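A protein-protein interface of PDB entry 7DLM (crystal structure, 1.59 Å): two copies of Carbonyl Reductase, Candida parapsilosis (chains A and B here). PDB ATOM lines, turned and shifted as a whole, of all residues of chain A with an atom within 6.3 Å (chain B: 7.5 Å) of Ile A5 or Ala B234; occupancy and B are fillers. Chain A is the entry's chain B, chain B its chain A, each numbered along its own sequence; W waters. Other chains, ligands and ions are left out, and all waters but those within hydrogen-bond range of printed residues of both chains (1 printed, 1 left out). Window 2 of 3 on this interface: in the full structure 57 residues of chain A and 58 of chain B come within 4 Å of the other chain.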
ATOM      1  N   GLY A   3      -5.760 -16.999   3.068  1.00  0.00           N
ATOM      2  CA  GLY A   3      -6.210 -18.286   3.557  1.00  0.00           C
ATOM      3  C   GLY A   3      -6.885 -18.237   4.907  1.00  0.00           C
ATOM      4  O   GLY A   3      -6.983 -19.265   5.583  1.00  0.00           O
ATOM      5  N   GLU A   4      -7.324 -17.064   5.338  1.00  0.00           N
ATOM      6  CA  GLU A   4      -8.161 -16.958   6.522  1.00  0.00           C
ATOM      7  C   GLU A   4      -9.423 -16.206   6.154  1.00  0.00           C
ATOM      8  O   GLU A   4      -9.377 -15.241   5.390  1.00  0.00           O
ATOM      9  CB  GLU A   4      -7.439 -16.257   7.681  1.00  0.00           C
ATOM     10  CG  GLU A   4      -6.012 -16.721   7.880  1.00  0.00           C
ATOM     11  CD  GLU A   4      -5.223 -15.812   8.797  1.00  0.00           C
ATOM     12  OE1 GLU A   4      -4.037 -16.118   9.054  1.00  0.00           O
ATOM     13  OE2 GLU A   4      -5.785 -14.794   9.259  1.00  0.00           O
ATOM     14  N   ILE A   5     -10.550 -16.682   6.659  1.00  0.00           N
ATOM     15  CA  ILE A   5     -11.779 -15.902   6.647  1.00  0.00           C
ATOM     16  C   ILE A   5     -11.678 -14.861   7.760  1.00  0.00           C
ATOM     17  O   ILE A   5     -11.730 -15.196   8.956  1.00  0.00           O
ATOM     18  CB  ILE A   5     -12.997 -16.813   6.843  1.00  0.00           C
ATOM     19  CG1 ILE A   5     -13.014 -17.919   5.778  1.00  0.00           C
ATOM     20  CG2 ILE A   5     -14.301 -16.013   6.725  1.00  0.00           C
ATOM     21  CD1 ILE A   5     -14.095 -18.954   5.944  1.00  0.00           C
ATOM     22  N   GLU A   6     -11.493 -13.595   7.370  1.00  0.00           N
ATOM     23  CA  GLU A   6     -11.609 -12.432   8.249  1.00  0.00           C
ATOM     24  C   GLU A   6     -13.017 -11.889   8.477  1.00  0.00           C
ATOM     25  O   GLU A   6     -13.804 -11.686   7.545  1.00  0.00           O
ATOM     26  CB  GLU A   6     -10.652 -11.297   7.724  1.00  0.00           C
ATOM     27  CG  GLU A   6     -11.067 -10.784   6.387  1.00  0.00           C
ATOM     28  CD  GLU A   6     -10.426 -11.629   5.235  1.00  0.00           C
ATOM     29  OE1 GLU A   6      -9.790 -12.702   5.049  1.00  0.00           O
ATOM     30  OE2 GLU A   6     -11.366 -11.879   4.527  1.00  0.00           O
ATOM     31  N   SER A   7     -13.265 -11.532   9.738  1.00  0.00           N
ATOM     32  CA  SER A   7     -14.524 -10.936  10.142  1.00  0.00           C
ATOM     33  C   SER A   7     -14.668  -9.529   9.582  1.00  0.00           C
ATOM     34  O   SER A   7     -13.719  -8.736   9.603  1.00  0.00           O
ATOM     35  CB  SER A   7     -14.616 -10.869  11.675  1.00  0.00           C
ATOM     36  OG  SER A   7     -15.839 -10.256  12.089  1.00  0.00           O
ATOM     37  N   GLY A  14     -10.116 -13.369  15.140  1.00  0.00           N
ATOM     38  CA  GLY A  14      -9.235 -14.318  14.498  1.00  0.00           C
ATOM     39  C   GLY A  14      -9.893 -14.985  13.312  1.00  0.00           C
ATOM     40  O   GLY A  14     -11.006 -14.637  12.919  1.00  0.00           O
ATOM     41  N   PRO A  15      -9.219 -15.965  12.713  1.00  0.00           N
ATOM     42  CA  PRO A  15      -9.792 -16.652  11.550  1.00  0.00           C
ATOM     43  C   PRO A  15     -11.123 -17.302  11.879  1.00  0.00           C
ATOM     44  O   PRO A  15     -11.294 -17.912  12.931  1.00  0.00           O
ATOM     45  CB  PRO A  15      -8.736 -17.710  11.200  1.00  0.00           C
ATOM     46  CG  PRO A  15      -7.496 -17.258  11.864  1.00  0.00           C
ATOM     47  CD  PRO A  15      -7.908 -16.522  13.100  1.00  0.00           C
ATOM     48  N   LEU A  16     -12.065 -17.189  10.954  1.00  0.00           N
ATOM     49  CA  LEU A  16     -13.408 -17.683  11.199  1.00  0.00           C
ATOM     50  C   LEU A  16     -13.586 -19.084  10.627  1.00  0.00           C
ATOM     51  O   LEU A  16     -12.845 -19.501   9.727  1.00  0.00           O
ATOM     52  CB  LEU A  16     -14.436 -16.729  10.570  1.00  0.00           C
ATOM     53  CG  LEU A  16     -14.422 -15.331  11.152  1.00  0.00           C
ATOM     54  CD1 LEU A  16     -15.538 -14.522  10.514  1.00  0.00           C
ATOM     55  CD2 LEU A  16     -14.568 -15.355  12.693  1.00  0.00           C
ATOM     56  N   PRO A  17     -14.567 -19.855  11.125  1.00  0.00           N
ATOM     57  CA  PRO A  17     -15.464 -19.522  12.247  1.00  0.00           C
ATOM     58  C   PRO A  17     -14.807 -19.686  13.614  1.00  0.00           C
ATOM     59  O   PRO A  17     -13.894 -20.507  13.765  1.00  0.00           O
ATOM     60  CB  PRO A  17     -16.604 -20.529  12.082  1.00  0.00           C
ATOM     61  CG  PRO A  17     -15.915 -21.756  11.553  1.00  0.00           C
ATOM     62  CD  PRO A  17     -14.814 -21.218  10.619  1.00  0.00           C
ATOM     63  N   SER B 229     -23.982 -22.950   0.286  1.00  0.00           N
ATOM     64  CA  SER B 229     -22.623 -23.305  -0.064  1.00  0.00           C
ATOM     65  C   SER B 229     -21.663 -22.812   1.009  1.00  0.00           C
ATOM     66  O   SER B 229     -22.025 -22.091   1.939  1.00  0.00           O
ATOM     67  CB  SER B 229     -22.217 -22.702  -1.397  1.00  0.00           C
ATOM     68  OG  SER B 229     -22.053 -21.306  -1.244  1.00  0.00           O
ATOM     69  N   LYS B 230     -20.403 -23.168   0.848  1.00  0.00           N
ATOM     70  CA  LYS B 230     -19.481 -22.899   1.936  1.00  0.00           C
ATOM     71  C   LYS B 230     -19.019 -21.441   1.883  1.00  0.00           C
ATOM     72  O   LYS B 230     -18.778 -20.823   2.925  1.00  0.00           O
ATOM     73  CB  LYS B 230     -18.411 -24.007   1.890  1.00  0.00           C
ATOM     74  CG  LYS B 230     -17.419 -24.109   3.059  1.00  0.00           C
ATOM     75  CD  LYS B 230     -16.091 -23.398   3.009  1.00  0.00           C
ATOM     76  CE  LYS B 230     -15.267 -23.762   4.246  1.00  0.00           C
ATOM     77  NZ  LYS B 230     -13.954 -23.052   4.221  1.00  0.00           N
ATOM     78  N   ASP B 231     -19.065 -20.846   0.694  1.00  0.00           N
ATOM     79  CA  ASP B 231     -18.824 -19.416   0.543  1.00  0.00           C
ATOM     80  C   ASP B 231     -19.993 -18.591   1.076  1.00  0.00           C
ATOM     81  O   ASP B 231     -19.789 -17.469   1.560  1.00  0.00           O
ATOM     82  CB  ASP B 231     -18.591 -19.062  -0.931  1.00  0.00           C
ATOM     83  CG  ASP B 231     -17.161 -19.323  -1.384  1.00  0.00           C
ATOM     84  OD1 ASP B 231     -16.266 -19.509  -0.535  1.00  0.00           O
ATOM     85  OD2 ASP B 231     -16.932 -19.330  -2.611  1.00  0.00           O
ATOM     86  N   MET B 232     -21.218 -19.121   0.964  1.00  0.00           N
ATOM     87  CA  MET B 232     -22.388 -18.482   1.557  1.00  0.00           C
ATOM     88  C   MET B 232     -22.290 -18.466   3.082  1.00  0.00           C
ATOM     89  O   MET B 232     -22.489 -17.425   3.718  1.00  0.00           O
ATOM     90  CB  MET B 232     -23.646 -19.224   1.111  1.00  0.00           C
ATOM     91  CG  MET B 232     -24.933 -18.650   1.656  1.00  0.00           C
ATOM     92  SD  MET B 232     -26.365 -19.411   0.877  1.00  0.00           S
ATOM     93  CE  MET B 232     -26.348 -18.583  -0.707  1.00  0.00           C
ATOM     94  N   LYS B 233     -21.990 -19.622   3.687  1.00  0.00           N
ATOM     95  CA  LYS B 233     -21.857 -19.683   5.140  1.00  0.00           C
ATOM     96  C   LYS B 233     -20.720 -18.794   5.627  1.00  0.00           C
ATOM     97  O   LYS B 233     -20.813 -18.189   6.704  1.00  0.00           O
ATOM     98  CB  LYS B 233     -21.643 -21.130   5.599  1.00  0.00           C
ATOM     99  CG  LYS B 233     -22.873 -22.043   5.567  1.00  0.00           C
ATOM    100  CD  LYS B 233     -22.534 -23.375   6.279  1.00  0.00           C
ATOM    101  CE  LYS B 233     -23.690 -24.369   6.314  1.00  0.00           C
ATOM    102  NZ  LYS B 233     -24.088 -24.739   7.720  1.00  0.00           N
ATOM    103  N   ALA B 234     -19.633 -18.706   4.852  1.00  0.00           N
ATOM    104  CA  ALA B 234     -18.513 -17.869   5.263  1.00  0.00           C
ATOM    105  C   ALA B 234     -18.937 -16.412   5.382  1.00  0.00           C
ATOM    106  O   ALA B 234     -18.482 -15.701   6.285  1.00  0.00           O
ATOM    107  CB  ALA B 234     -17.360 -18.014   4.270  1.00  0.00           C
ATOM    108  N   LYS B 235     -19.804 -15.945   4.478  1.00  0.00           N
ATOM    109  CA  LYS B 235     -20.276 -14.566   4.581  1.00  0.00           C
ATOM    110  C   LYS B 235     -21.176 -14.375   5.795  1.00  0.00           C
ATOM    111  O   LYS B 235     -21.091 -13.338   6.468  1.00  0.00           O
ATOM    112  CB  LYS B 235     -20.998 -14.146   3.300  1.00  0.00           C
ATOM    113  CG  LYS B 235     -20.073 -14.190   2.078  1.00  0.00           C
ATOM    114  CD  LYS B 235     -20.770 -13.616   0.851  1.00  0.00           C
ATOM    115  CE  LYS B 235     -19.815 -13.493  -0.342  1.00  0.00           C
ATOM    116  NZ  LYS B 235     -19.387 -14.833  -0.858  1.00  0.00           N
ATOM    117  N   TRP B 236     -22.021 -15.363   6.116  1.00  0.00           N
ATOM    118  CA  TRP B 236     -22.776 -15.286   7.368  1.00  0.00           C
ATOM    119  C   TRP B 236     -21.838 -15.122   8.559  1.00  0.00           C
ATOM    120  O   TRP B 236     -22.063 -14.277   9.427  1.00  0.00           O
ATOM    121  CB  TRP B 236     -23.646 -16.531   7.577  1.00  0.00           C
ATOM    122  CG  TRP B 236     -24.664 -16.879   6.498  1.00  0.00           C
ATOM    123  CD1 TRP B 236     -25.131 -16.077   5.484  1.00  0.00           C
ATOM    124  CD2 TRP B 236     -25.345 -18.128   6.368  1.00  0.00           C
ATOM    125  NE1 TRP B 236     -26.062 -16.770   4.721  1.00  0.00           N
ATOM    126  CE2 TRP B 236     -26.200 -18.031   5.245  1.00  0.00           C
ATOM    127  CE3 TRP B 236     -25.309 -19.328   7.091  1.00  0.00           C
ATOM    128  CZ2 TRP B 236     -27.021 -19.086   4.838  1.00  0.00           C
ATOM    129  CZ3 TRP B 236     -26.118 -20.373   6.685  1.00  0.00           C
ATOM    130  CH2 TRP B 236     -26.962 -20.247   5.567  1.00  0.00           C
ATOM    131  N   TRP B 237     -20.778 -15.932   8.619  1.00  0.00           N
ATOM    132  CA  TRP B 237     -19.843 -15.827   9.732  1.00  0.00           C
ATOM    133  C   TRP B 237     -19.213 -14.440   9.799  1.00  0.00           C
ATOM    134  O   TRP B 237     -19.059 -13.872  10.892  1.00  0.00           O
ATOM    135  CB  TRP B 237     -18.747 -16.886   9.604  1.00  0.00           C
ATOM    136  CG  TRP B 237     -19.218 -18.306   9.485  1.00  0.00           C
ATOM    137  CD1 TRP B 237     -20.416 -18.831   9.907  1.00  0.00           C
ATOM    138  CD2 TRP B 237     -18.482 -19.393   8.915  1.00  0.00           C
ATOM    139  NE1 TRP B 237     -20.470 -20.178   9.607  1.00  0.00           N
ATOM    140  CE2 TRP B 237     -19.294 -20.547   9.006  1.00  0.00           C
ATOM    141  CE3 TRP B 237     -17.217 -19.499   8.316  1.00  0.00           C
ATOM    142  CZ2 TRP B 237     -18.881 -21.795   8.526  1.00  0.00           C
ATOM    143  CZ3 TRP B 237     -16.812 -20.740   7.832  1.00  0.00           C
ATOM    144  CH2 TRP B 237     -17.636 -21.873   7.955  1.00  0.00           C
ATOM    145  N   GLN B 238     -18.839 -13.879   8.632  1.00  0.00           N
ATOM    146  CA  GLN B 238     -18.198 -12.566   8.595  1.00  0.00           C
ATOM    147  C   GLN B 238     -19.100 -11.474   9.151  1.00  0.00           C
ATOM    148  O   GLN B 238     -18.607 -10.473   9.684  1.00  0.00           O
ATOM    149  CB  GLN B 238     -17.805 -12.205   7.159  1.00  0.00           C
ATOM    150  CG  GLN B 238     -16.639 -13.068   6.607  1.00  0.00           C
ATOM    151  CD  GLN B 238     -16.239 -12.636   5.212  1.00  0.00           C
ATOM    152  OE1 GLN B 238     -17.068 -12.588   4.316  1.00  0.00           O
ATOM    153  NE2 GLN B 238     -14.966 -12.297   5.029  1.00  0.00           N
ATOM    154  N   LEU B 239     -20.416 -11.649   9.026  1.00  0.00           N
ATOM    155  CA  LEU B 239     -21.391 -10.655   9.446  1.00  0.00           C
ATOM    156  C   LEU B 239     -21.960 -10.925  10.841  1.00  0.00           C
ATOM    157  O   LEU B 239     -22.760 -10.125  11.331  1.00  0.00           O
ATOM    158  CB  LEU B 239     -22.529 -10.585   8.408  1.00  0.00           C
ATOM    159  CG  LEU B 239     -22.111 -10.127   6.998  1.00  0.00           C
ATOM    160  CD1 LEU B 239     -23.324 -10.001   6.057  1.00  0.00           C
ATOM    161  CD2 LEU B 239     -21.371  -8.823   7.072  1.00  0.00           C
ATOM    162  N   THR B 240     -21.571 -12.029  11.496  1.00  0.00           N
ATOM    163  CA  THR B 240     -22.060 -12.364  12.835  1.00  0.00           C
ATOM    164  C   THR B 240     -21.066 -11.892  13.888  1.00  0.00           C
ATOM    165  O   THR B 240     -19.918 -12.371  13.889  1.00  0.00           O
ATOM    166  CB  THR B 240     -22.258 -13.875  12.965  1.00  0.00           C
ATOM    167  OG1 THR B 240     -23.139 -14.356  11.938  1.00  0.00           O
ATOM    168  CG2 THR B 240     -22.880 -14.201  14.348  1.00  0.00           C
ATOM    169  N   GLY B 243     -19.021 -14.580  15.370  1.00  0.00           N
ATOM    170  CA  GLY B 243     -18.110 -15.170  14.401  1.00  0.00           C
ATOM    171  C   GLY B 243     -18.398 -16.592  13.981  1.00  0.00           C
ATOM    172  O   GLY B 243     -17.501 -17.242  13.422  1.00  0.00           O
ATOM    173  N   GLU B 245     -21.877 -19.866  13.488  1.00  0.00           N
ATOM    174  CA  GLU B 245     -23.235 -20.335  13.712  1.00  0.00           C
ATOM    175  C   GLU B 245     -23.412 -20.804  15.153  1.00  0.00           C
ATOM    176  O   GLU B 245     -22.451 -21.108  15.861  1.00  0.00           O
ATOM    177  CB  GLU B 245     -23.576 -21.474  12.754  1.00  0.00           C
ATOM    178  CG  GLU B 245     -23.573 -21.060  11.292  1.00  0.00           C
ATOM    179  CD  GLU B 245     -23.404 -22.242  10.363  1.00  0.00           C
ATOM    180  OE1 GLU B 245     -22.301 -22.386   9.793  1.00  0.00           O
ATOM    181  OE2 GLU B 245     -24.369 -23.022  10.200  1.00  0.00           O
HETATM  182  O   HOH W   1     -13.450 -11.799   2.478  1.00  0.00           O
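Water W1 lies within hydrogen-bond range of the side-chain carboxylate of Glu A6 (2.9 Å) and the side-chain amide nitrogen of Gln B238 (3.0 Å).
The side-chain carboxylate (OE1) of Glu B245 sits at hydrogen-bond distance from the indole nitrogen (NE1) of Trp B237 (2.9 Å). The backbone carbonyl oxygen of Glu A4 lies close to the side-chain carboxylate of Glu A6, 2.6 Å away. N of Leu A16 is in hydrogen-bond range of O of Ile A5.
Of the 14 printed residues of chain B, 4 touch a printed residue of chain A. Printed residues of chain B that touch a printed residue of chain A: Ala B234, Trp B237, Gln B238 and Gly B243. Of the 9 printed residues of chain A, 5 touch a printed residue of chain B. Printed residues of chain A that touch a printed residue of chain B: Ile A5, Glu A6, Ser A7, Leu A16 and Pro A17. Among the printed residues, no Asp or Glu carboxylate lies within 4 Å of a Lys or Arg side-chain nitrogen of the other chain.
Ile A5 touches just these residues of chain B: Ala B234, Trp B237 and Gln B238. Of chain A, only Ile A5 comes within 4 Å of Ala B234. Printed residues of chain B within 4 Å of Glu A6: Gln B238 (2.8 Å). Of the printed residues of chain A, Gly B243 touches Leu A16 and Pro A17. The nearest residue of chain B that does not touch Ile A5 is Lys B230 (4.4 Å). The nearest residue of chain A that does not touch Ala B234 is Leu A16 (5.3 Å). The nearest printed residue of chain A that does not touch Gly B243 is Ser A7 (5.9 Å).
The backbone carbonyl oxygen (O) of Glu A6 sits at hydrogen-bond distance from the side-chain amide nitrogen (NE2) of Gln B238, at 2.8 Å.
Among the printed residues, pairs that only touch across the chains: Ile A5 with Ala B234, Ile A5 with Trp B237, Ile A5 with Gln B238, Ser A7 with Gln B238, Leu A16 with Trp B237, Leu A16 with Gln B238, Leu A16 with Gly B243, Pro A17 with Trp B237 and Pro A17 with Gly B243.
No position is printed for both chains. Of the 10 pairs that touch across the chains among the printed residues, none has its exchanged pair printed and touching as well.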
